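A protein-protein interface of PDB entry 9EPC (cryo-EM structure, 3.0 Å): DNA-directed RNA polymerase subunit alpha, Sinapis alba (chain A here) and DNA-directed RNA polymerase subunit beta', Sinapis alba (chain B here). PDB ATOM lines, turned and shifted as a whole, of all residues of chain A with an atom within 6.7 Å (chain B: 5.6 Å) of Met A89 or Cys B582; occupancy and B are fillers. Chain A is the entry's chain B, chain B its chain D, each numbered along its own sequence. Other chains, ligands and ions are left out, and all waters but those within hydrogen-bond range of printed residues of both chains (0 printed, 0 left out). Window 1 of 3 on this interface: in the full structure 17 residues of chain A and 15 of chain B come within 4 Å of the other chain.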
ATOM      1  N   VAL A  84       6.443 -28.678 -18.025  1.00  0.00           N
ATOM      2  CA  VAL A  84       5.232 -29.447 -17.761  1.00  0.00           C
ATOM      3  C   VAL A  84       4.594 -28.999 -16.455  1.00  0.00           C
ATOM      4  O   VAL A  84       3.371 -28.844 -16.364  1.00  0.00           O
ATOM      5  CB  VAL A  84       5.546 -30.953 -17.753  1.00  0.00           C
ATOM      6  CG1 VAL A  84       4.318 -31.742 -17.351  1.00  0.00           C
ATOM      7  CG2 VAL A  84       6.039 -31.393 -19.119  1.00  0.00           C
ATOM      8  N   HIS A  85       5.412 -28.778 -15.425  1.00  0.00           N
ATOM      9  CA  HIS A  85       4.882 -28.323 -14.145  1.00  0.00           C
ATOM     10  C   HIS A  85       4.242 -26.946 -14.269  1.00  0.00           C
ATOM     11  O   HIS A  85       3.209 -26.676 -13.645  1.00  0.00           O
ATOM     12  CB  HIS A  85       5.991 -28.308 -13.098  1.00  0.00           C
ATOM     13  CG  HIS A  85       5.527 -27.921 -11.731  1.00  0.00           C
ATOM     14  ND1 HIS A  85       5.939 -26.764 -11.106  1.00  0.00           N
ATOM     15  CD2 HIS A  85       4.687 -28.536 -10.867  1.00  0.00           C
ATOM     16  CE1 HIS A  85       5.374 -26.684  -9.916  1.00  0.00           C
ATOM     17  NE2 HIS A  85       4.608 -27.746  -9.747  1.00  0.00           N
ATOM     18  N   GLU A  86       4.841 -26.057 -15.063  1.00  0.00           N
ATOM     19  CA  GLU A  86       4.265 -24.729 -15.239  1.00  0.00           C
ATOM     20  C   GLU A  86       2.975 -24.772 -16.044  1.00  0.00           C
ATOM     21  O   GLU A  86       2.081 -23.949 -15.819  1.00  0.00           O
ATOM     22  CB  GLU A  86       5.272 -23.795 -15.904  1.00  0.00           C
ATOM     23  CG  GLU A  86       6.233 -23.119 -14.937  1.00  0.00           C
ATOM     24  CD  GLU A  86       5.549 -22.125 -14.014  1.00  0.00           C
ATOM     25  OE1 GLU A  86       4.892 -22.557 -13.044  1.00  0.00           O
ATOM     26  OE2 GLU A  86       5.665 -20.907 -14.263  1.00  0.00           O
ATOM     27  N   ILE A  87       2.861 -25.706 -16.990  1.00  0.00           N
ATOM     28  CA  ILE A  87       1.614 -25.849 -17.735  1.00  0.00           C
ATOM     29  C   ILE A  87       0.481 -26.231 -16.794  1.00  0.00           C
ATOM     30  O   ILE A  87      -0.630 -25.696 -16.887  1.00  0.00           O
ATOM     31  CB  ILE A  87       1.781 -26.873 -18.871  1.00  0.00           C
ATOM     32  CG1 ILE A  87       2.695 -26.308 -19.958  1.00  0.00           C
ATOM     33  CG2 ILE A  87       0.432 -27.246 -19.453  1.00  0.00           C
ATOM     34  CD1 ILE A  87       2.895 -27.241 -21.125  1.00  0.00           C
ATOM     35  N   LEU A  88       0.746 -27.153 -15.866  1.00  0.00           N
ATOM     36  CA  LEU A  88      -0.253 -27.493 -14.861  1.00  0.00           C
ATOM     37  C   LEU A  88      -0.615 -26.279 -14.019  1.00  0.00           C
ATOM     38  O   LEU A  88      -1.784 -26.082 -13.668  1.00  0.00           O
ATOM     39  CB  LEU A  88       0.260 -28.621 -13.970  1.00  0.00           C
ATOM     40  CG  LEU A  88       0.754 -29.882 -14.673  1.00  0.00           C
ATOM     41  CD1 LEU A  88       1.157 -30.923 -13.647  1.00  0.00           C
ATOM     42  CD2 LEU A  88      -0.308 -30.428 -15.606  1.00  0.00           C
ATOM     43  N   MET A  89       0.379 -25.455 -13.681  1.00  0.00           N
ATOM     44  CA  MET A  89       0.107 -24.250 -12.909  1.00  0.00           C
ATOM     45  C   MET A  89      -0.791 -23.294 -13.682  1.00  0.00           C
ATOM     46  O   MET A  89      -1.702 -22.687 -13.110  1.00  0.00           O
ATOM     47  CB  MET A  89       1.419 -23.567 -12.529  1.00  0.00           C
ATOM     48  CG  MET A  89       1.361 -22.814 -11.218  1.00  0.00           C
ATOM     49  SD  MET A  89       1.019 -23.916  -9.836  1.00  0.00           S
ATOM     50  CE  MET A  89       2.377 -25.066  -9.993  1.00  0.00           C
ATOM     51  N   ASN A  90      -0.543 -23.142 -14.984  1.00  0.00           N
ATOM     52  CA  ASN A  90      -1.404 -22.296 -15.803  1.00  0.00           C
ATOM     53  C   ASN A  90      -2.809 -22.874 -15.908  1.00  0.00           C
ATOM     54  O   ASN A  90      -3.794 -22.129 -15.891  1.00  0.00           O
ATOM     55  CB  ASN A  90      -0.792 -22.114 -17.189  1.00  0.00           C
ATOM     56  CG  ASN A  90       0.506 -21.345 -17.150  1.00  0.00           C
ATOM     57  OD1 ASN A  90       0.718 -20.510 -16.271  1.00  0.00           O
ATOM     58  ND2 ASN A  90       1.386 -21.620 -18.102  1.00  0.00           N
ATOM     59  N   LEU A  91      -2.920 -24.200 -16.024  1.00  0.00           N
ATOM     60  CA  LEU A  91      -4.235 -24.829 -16.064  1.00  0.00           C
ATOM     61  C   LEU A  91      -4.991 -24.603 -14.764  1.00  0.00           C
ATOM     62  O   LEU A  91      -6.207 -24.379 -14.775  1.00  0.00           O
ATOM     63  CB  LEU A  91      -4.092 -26.322 -16.346  1.00  0.00           C
ATOM     64  CG  LEU A  91      -3.614 -26.713 -17.742  1.00  0.00           C
ATOM     65  CD1 LEU A  91      -3.348 -28.203 -17.807  1.00  0.00           C
ATOM     66  CD2 LEU A  91      -4.639 -26.311 -18.780  1.00  0.00           C
ATOM     67  N   ASN A  92      -4.287 -24.656 -13.633  1.00  0.00           N
ATOM     68  CA  ASN A  92      -4.925 -24.456 -12.338  1.00  0.00           C
ATOM     69  C   ASN A  92      -5.519 -23.063 -12.194  1.00  0.00           C
ATOM     70  O   ASN A  92      -6.431 -22.870 -11.385  1.00  0.00           O
ATOM     71  CB  ASN A  92      -3.914 -24.712 -11.221  1.00  0.00           C
ATOM     72  CG  ASN A  92      -4.558 -24.786  -9.857  1.00  0.00           C
ATOM     73  OD1 ASN A  92      -5.755 -25.040  -9.735  1.00  0.00           O
ATOM     74  ND2 ASN A  92      -3.763 -24.568  -8.818  1.00  0.00           N
ATOM     75  N   GLU A  93      -5.031 -22.090 -12.959  1.00  0.00           N
ATOM     76  CA  GLU A  93      -5.546 -20.731 -12.892  1.00  0.00           C
ATOM     77  C   GLU A  93      -6.749 -20.501 -13.795  1.00  0.00           C
ATOM     78  O   GLU A  93      -7.330 -19.413 -13.754  1.00  0.00           O
ATOM     79  CB  GLU A  93      -4.447 -19.731 -13.260  1.00  0.00           C
ATOM     80  CG  GLU A  93      -3.247 -19.759 -12.336  1.00  0.00           C
ATOM     81  CD  GLU A  93      -2.160 -18.798 -12.766  1.00  0.00           C
ATOM     82  OE1 GLU A  93      -2.248 -18.264 -13.891  1.00  0.00           O
ATOM     83  OE2 GLU A  93      -1.217 -18.572 -11.978  1.00  0.00           O
ATOM     84  N   ILE A  94      -7.132 -21.487 -14.604  1.00  0.00           N
ATOM     85  CA  ILE A  94      -8.259 -21.312 -15.509  1.00  0.00           C
ATOM     86  C   ILE A  94      -9.547 -21.228 -14.705  1.00  0.00           C
ATOM     87  O   ILE A  94      -9.827 -22.082 -13.855  1.00  0.00           O
ATOM     88  CB  ILE A  94      -8.315 -22.458 -16.529  1.00  0.00           C
ATOM     89  CG1 ILE A  94      -7.086 -22.416 -17.430  1.00  0.00           C
ATOM     90  CG2 ILE A  94      -9.570 -22.355 -17.368  1.00  0.00           C
ATOM     91  CD1 ILE A  94      -6.968 -21.133 -18.197  1.00  0.00           C
ATOM     92  N   ILE A 172      -4.019 -32.040 -10.679  1.00  0.00           N
ATOM     93  CA  ILE A 172      -3.940 -30.605 -10.445  1.00  0.00           C
ATOM     94  C   ILE A 172      -4.650 -30.314  -9.134  1.00  0.00           C
ATOM     95  O   ILE A 172      -5.857 -30.555  -9.010  1.00  0.00           O
ATOM     96  CB  ILE A 172      -4.562 -29.803 -11.598  1.00  0.00           C
ATOM     97  CG1 ILE A 172      -3.802 -30.066 -12.895  1.00  0.00           C
ATOM     98  CG2 ILE A 172      -4.567 -28.325 -11.270  1.00  0.00           C
ATOM     99  CD1 ILE A 172      -4.313 -29.270 -14.066  1.00  0.00           C
ATOM    100  N   PHE B 580       1.387 -26.817  -4.036  1.00  0.00           N
ATOM    101  CA  PHE B 580       1.905 -25.705  -4.819  1.00  0.00           C
ATOM    102  C   PHE B 580       0.750 -24.769  -5.135  1.00  0.00           C
ATOM    103  O   PHE B 580      -0.255 -25.193  -5.713  1.00  0.00           O
ATOM    104  CB  PHE B 580       2.558 -26.194  -6.111  1.00  0.00           C
ATOM    105  CG  PHE B 580       3.962 -26.686  -5.933  1.00  0.00           C
ATOM    106  CD1 PHE B 580       4.215 -27.887  -5.299  1.00  0.00           C
ATOM    107  CD2 PHE B 580       5.030 -25.953  -6.418  1.00  0.00           C
ATOM    108  CE1 PHE B 580       5.509 -28.342  -5.141  1.00  0.00           C
ATOM    109  CE2 PHE B 580       6.324 -26.404  -6.264  1.00  0.00           C
ATOM    110  CZ  PHE B 580       6.563 -27.599  -5.625  1.00  0.00           C
ATOM    111  N   PHE B 581       0.892 -23.503  -4.759  1.00  0.00           N
ATOM    112  CA  PHE B 581      -0.133 -22.498  -4.996  1.00  0.00           C
ATOM    113  C   PHE B 581       0.365 -21.500  -6.029  1.00  0.00           C
ATOM    114  O   PHE B 581       1.469 -20.963  -5.899  1.00  0.00           O
ATOM    115  CB  PHE B 581      -0.510 -21.787  -3.697  1.00  0.00           C
ATOM    116  CG  PHE B 581      -1.160 -22.684  -2.692  1.00  0.00           C
ATOM    117  CD1 PHE B 581      -2.486 -23.043  -2.827  1.00  0.00           C
ATOM    118  CD2 PHE B 581      -0.445 -23.176  -1.619  1.00  0.00           C
ATOM    119  CE1 PHE B 581      -3.088 -23.872  -1.909  1.00  0.00           C
ATOM    120  CE2 PHE B 581      -1.044 -24.006  -0.697  1.00  0.00           C
ATOM    121  CZ  PHE B 581      -2.366 -24.354  -0.843  1.00  0.00           C
ATOM    122  N   CYS B 582      -0.451 -21.260  -7.055  1.00  0.00           N
ATOM    123  CA  CYS B 582      -0.057 -20.359  -8.128  1.00  0.00           C
ATOM    124  C   CYS B 582       0.015 -18.909  -7.676  1.00  0.00           C
ATOM    125  O   CYS B 582       0.752 -18.122  -8.278  1.00  0.00           O
ATOM    126  CB  CYS B 582      -1.026 -20.495  -9.299  1.00  0.00           C
ATOM    127  SG  CYS B 582      -2.759 -20.288  -8.843  1.00  0.00           S
ATOM    128  N   ASN B 583      -0.728 -18.536  -6.637  1.00  0.00           N
ATOM    129  CA  ASN B 583      -0.695 -17.174  -6.129  1.00  0.00           C
ATOM    130  C   ASN B 583      -1.098 -17.185  -4.664  1.00  0.00           C
ATOM    131  O   ASN B 583      -1.668 -18.156  -4.162  1.00  0.00           O
ATOM    132  CB  ASN B 583      -1.610 -16.246  -6.935  1.00  0.00           C
ATOM    133  CG  ASN B 583      -2.963 -16.858  -7.203  1.00  0.00           C
ATOM    134  OD1 ASN B 583      -3.326 -17.867  -6.605  1.00  0.00           O
ATOM    135  ND2 ASN B 583      -3.718 -16.251  -8.110  1.00  0.00           N
ATOM    136  N   SER B 584      -0.788 -16.083  -3.979  1.00  0.00           N
ATOM    137  CA  SER B 584      -1.036 -16.009  -2.545  1.00  0.00           C
ATOM    138  C   SER B 584      -2.521 -16.070  -2.219  1.00  0.00           C
ATOM    139  O   SER B 584      -2.897 -16.500  -1.124  1.00  0.00           O
ATOM    140  CB  SER B 584      -0.421 -14.733  -1.976  1.00  0.00           C
ATOM    141  OG  SER B 584      -0.946 -13.589  -2.622  1.00  0.00           O
ATOM    142  N   ASP B 586      -4.824 -18.017  -3.539  1.00  0.00           N
ATOM    143  CA  ASP B 586      -5.219 -19.414  -3.391  1.00  0.00           C
ATOM    144  C   ASP B 586      -4.720 -19.992  -2.075  1.00  0.00           C
ATOM    145  O   ASP B 586      -5.428 -20.771  -1.427  1.00  0.00           O
ATOM    146  CB  ASP B 586      -4.703 -20.237  -4.567  1.00  0.00           C
ATOM    147  CG  ASP B 586      -5.399 -19.892  -5.863  1.00  0.00           C
ATOM    148  OD1 ASP B 586      -6.146 -18.894  -5.886  1.00  0.00           O
ATOM    149  OD2 ASP B 586      -5.202 -20.619  -6.858  1.00  0.00           O
ATOM    150  N   TRP B 603       4.357 -24.323  -1.123  1.00  0.00           N
ATOM    151  CA  TRP B 603       5.162 -23.671  -2.143  1.00  0.00           C
ATOM    152  C   TRP B 603       4.323 -22.613  -2.840  1.00  0.00           C
ATOM    153  O   TRP B 603       3.228 -22.906  -3.330  1.00  0.00           O
ATOM    154  CB  TRP B 603       5.688 -24.683  -3.158  1.00  0.00           C
ATOM    155  CG  TRP B 603       6.679 -25.626  -2.581  1.00  0.00           C
ATOM    156  CD1 TRP B 603       6.419 -26.822  -1.986  1.00  0.00           C
ATOM    157  CD2 TRP B 603       8.096 -25.455  -2.540  1.00  0.00           C
ATOM    158  NE1 TRP B 603       7.589 -27.409  -1.577  1.00  0.00           N
ATOM    159  CE2 TRP B 603       8.635 -26.588  -1.906  1.00  0.00           C
ATOM    160  CE3 TRP B 603       8.964 -24.453  -2.978  1.00  0.00           C
ATOM    161  CZ2 TRP B 603       9.998 -26.748  -1.700  1.00  0.00           C
ATOM    162  CZ3 TRP B 603      10.317 -24.614  -2.773  1.00  0.00           C
ATOM    163  CH2 TRP B 603      10.822 -25.752  -2.141  1.00  0.00           C
ATOM    164  N   LEU B 604       4.839 -21.392  -2.885  1.00  0.00           N
ATOM    165  CA  LEU B 604       4.151 -20.263  -3.491  1.00  0.00           C
ATOM    166  C   LEU B 604       4.871 -19.891  -4.777  1.00  0.00           C
ATOM    167  O   LEU B 604       6.073 -19.610  -4.757  1.00  0.00           O
ATOM    168  CB  LEU B 604       4.113 -19.075  -2.535  1.00  0.00           C
ATOM    169  CG  LEU B 604       3.298 -17.870  -2.995  1.00  0.00           C
ATOM    170  CD1 LEU B 604       1.837 -18.245  -3.101  1.00  0.00           C
ATOM    171  CD2 LEU B 604       3.490 -16.707  -2.041  1.00  0.00           C
ATOM    172  N   ARG B 605       4.143 -19.890  -5.888  1.00  0.00           N
ATOM    173  CA  ARG B 605       4.725 -19.499  -7.165  1.00  0.00           C
ATOM    174  C   ARG B 605       4.985 -17.999  -7.146  1.00  0.00           C
ATOM    175  O   ARG B 605       4.048 -17.197  -7.188  1.00  0.00           O
ATOM    176  CB  ARG B 605       3.801 -19.885  -8.315  1.00  0.00           C
ATOM    177  CG  ARG B 605       4.484 -19.895  -9.666  1.00  0.00           C
ATOM    178  CD  ARG B 605       4.042 -18.731 -10.523  1.00  0.00           C
ATOM    179  NE  ARG B 605       2.642 -18.848 -10.911  1.00  0.00           N
ATOM    180  CZ  ARG B 605       2.217 -19.492 -11.989  1.00  0.00           C
ATOM    181  NH1 ARG B 605       3.059 -20.096 -12.810  1.00  0.00           N
ATOM    182  NH2 ARG B 605       0.914 -19.532 -12.248  1.00  0.00           N
ATOM    183  N   GLN B 607       5.990 -14.533  -8.510  1.00  0.00           N
ATOM    184  CA  GLN B 607       6.043 -13.811  -9.772  1.00  0.00           C
ATOM    185  C   GLN B 607       6.959 -12.600  -9.727  1.00  0.00           C
ATOM    186  O   GLN B 607       7.416 -12.147 -10.782  1.00  0.00           O
ATOM    187  CB  GLN B 607       4.637 -13.361 -10.181  1.00  0.00           C
ATOM    188  CG  GLN B 607       3.623 -14.489 -10.314  1.00  0.00           C
ATOM    189  CD  GLN B 607       3.768 -15.272 -11.607  1.00  0.00           C
ATOM    190  OE1 GLN B 607       4.797 -15.206 -12.279  1.00  0.00           O
ATOM    191  NE2 GLN B 607       2.728 -16.013 -11.965  1.00  0.00           N
ATOM    192  N   TYR B 651       9.838 -20.463  -6.788  1.00  0.00           N
ATOM    193  CA  TYR B 651       8.830 -20.988  -5.876  1.00  0.00           C
ATOM    194  C   TYR B 651       9.341 -20.817  -4.455  1.00  0.00           C
ATOM    195  O   TYR B 651      10.422 -21.309  -4.120  1.00  0.00           O
ATOM    196  CB  TYR B 651       8.532 -22.458  -6.166  1.00  0.00           C
ATOM    197  CG  TYR B 651       7.983 -22.701  -7.546  1.00  0.00           C
ATOM    198  CD1 TYR B 651       8.830 -22.880  -8.628  1.00  0.00           C
ATOM    199  CD2 TYR B 651       6.617 -22.751  -7.770  1.00  0.00           C
ATOM    200  CE1 TYR B 651       8.334 -23.101  -9.890  1.00  0.00           C
ATOM    201  CE2 TYR B 651       6.112 -22.971  -9.028  1.00  0.00           C
ATOM    202  CZ  TYR B 651       6.975 -23.145 -10.087  1.00  0.00           C
ATOM    203  OH  TYR B 651       6.472 -23.366 -11.346  1.00  0.00           O
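OH of Tyr B651 lies within hydrogen-bond range of ND1 of His A85, at 3.4 Å.
The guanidinium group (NH1) of Arg B605 is in salt-bridge range of the side-chain carboxylate (OE1) of Glu A86.
The side-chain hydroxyl (OH) of Tyr B651 lies within hydrogen-bond range of the side-chain carboxylate (OE1) of Glu A86, at 2.5 Å.
OE1 of Glu A93 lies within salt-bridge range of NH2 of Arg B605 (3.8 Å).
The backbone carbonyl oxygen (O) of Glu A86 sits close to the side-chain amide nitrogen (ND2) of Asn A90, at 3.3 Å.
The backbone NH (N) of Arg B605 lies within hydrogen-bond range of the backbone carbonyl oxygen (O) of Phe B581.
SG of Cys B582 sits at hydrogen-bond distance from OD1 of Asn B583 (3.3 Å).
OD2 of Asp B586 sits at hydrogen-bond distance from SG of Cys B582 (3.2 Å).
O of Cys B582 is in hydrogen-bond range of NE of Arg B605, 3.3 Å away.
NE2 of Gln B607 sits close to NE of Arg B605, 3.0 Å away.
His A85 touches Phe B580 (CE1 to CD2, 3.6 Å).
CB of Cys B582 touches CG of Met A89, at 3.8 Å.
Met A89 touches Arg B605 (CG to NH2, 3.5 Å).
Glu A93 touches Cys B582.
Of the printed residues of chain B, His A85 touches Phe B580 and Tyr B651.
Printed residues of chain B within 4 Å of Glu A86: Arg B605 and Tyr B651.
Met A89 touches just these residues of chain B: Cys B582 (3.8 Å) and Arg B605 (3.5 Å).
Cys B582 touches just these residues of chain A: Met A89 and Glu A93.
Trp B603 touches none of the printed residues of chain A.
Of the printed residues of chain A, Arg B605 touches Glu A86, Met A89 and Glu A93.
The nearest residue of chain B that does not touch Met A89 is Phe B580 (4.05 Å).
The nearest residue of chain A that does not touch Cys B582 is Asn A92 (4.4 Å).
Of the 12 printed residues of chain A, 4 touch a printed residue of chain B.
Of the 11 printed residues of chain B, 4 touch a printed residue of chain A.
Printed residues of chain B that touch a printed residue of chain A: Phe B580, Cys B582, Arg B605 and Tyr B651.
Hydrophobic or aromatic side chains of chain B that line the printed part of chain A: Phe B580 and Tyr B651.
Among the printed residues, 8 pairs touch across the chains.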
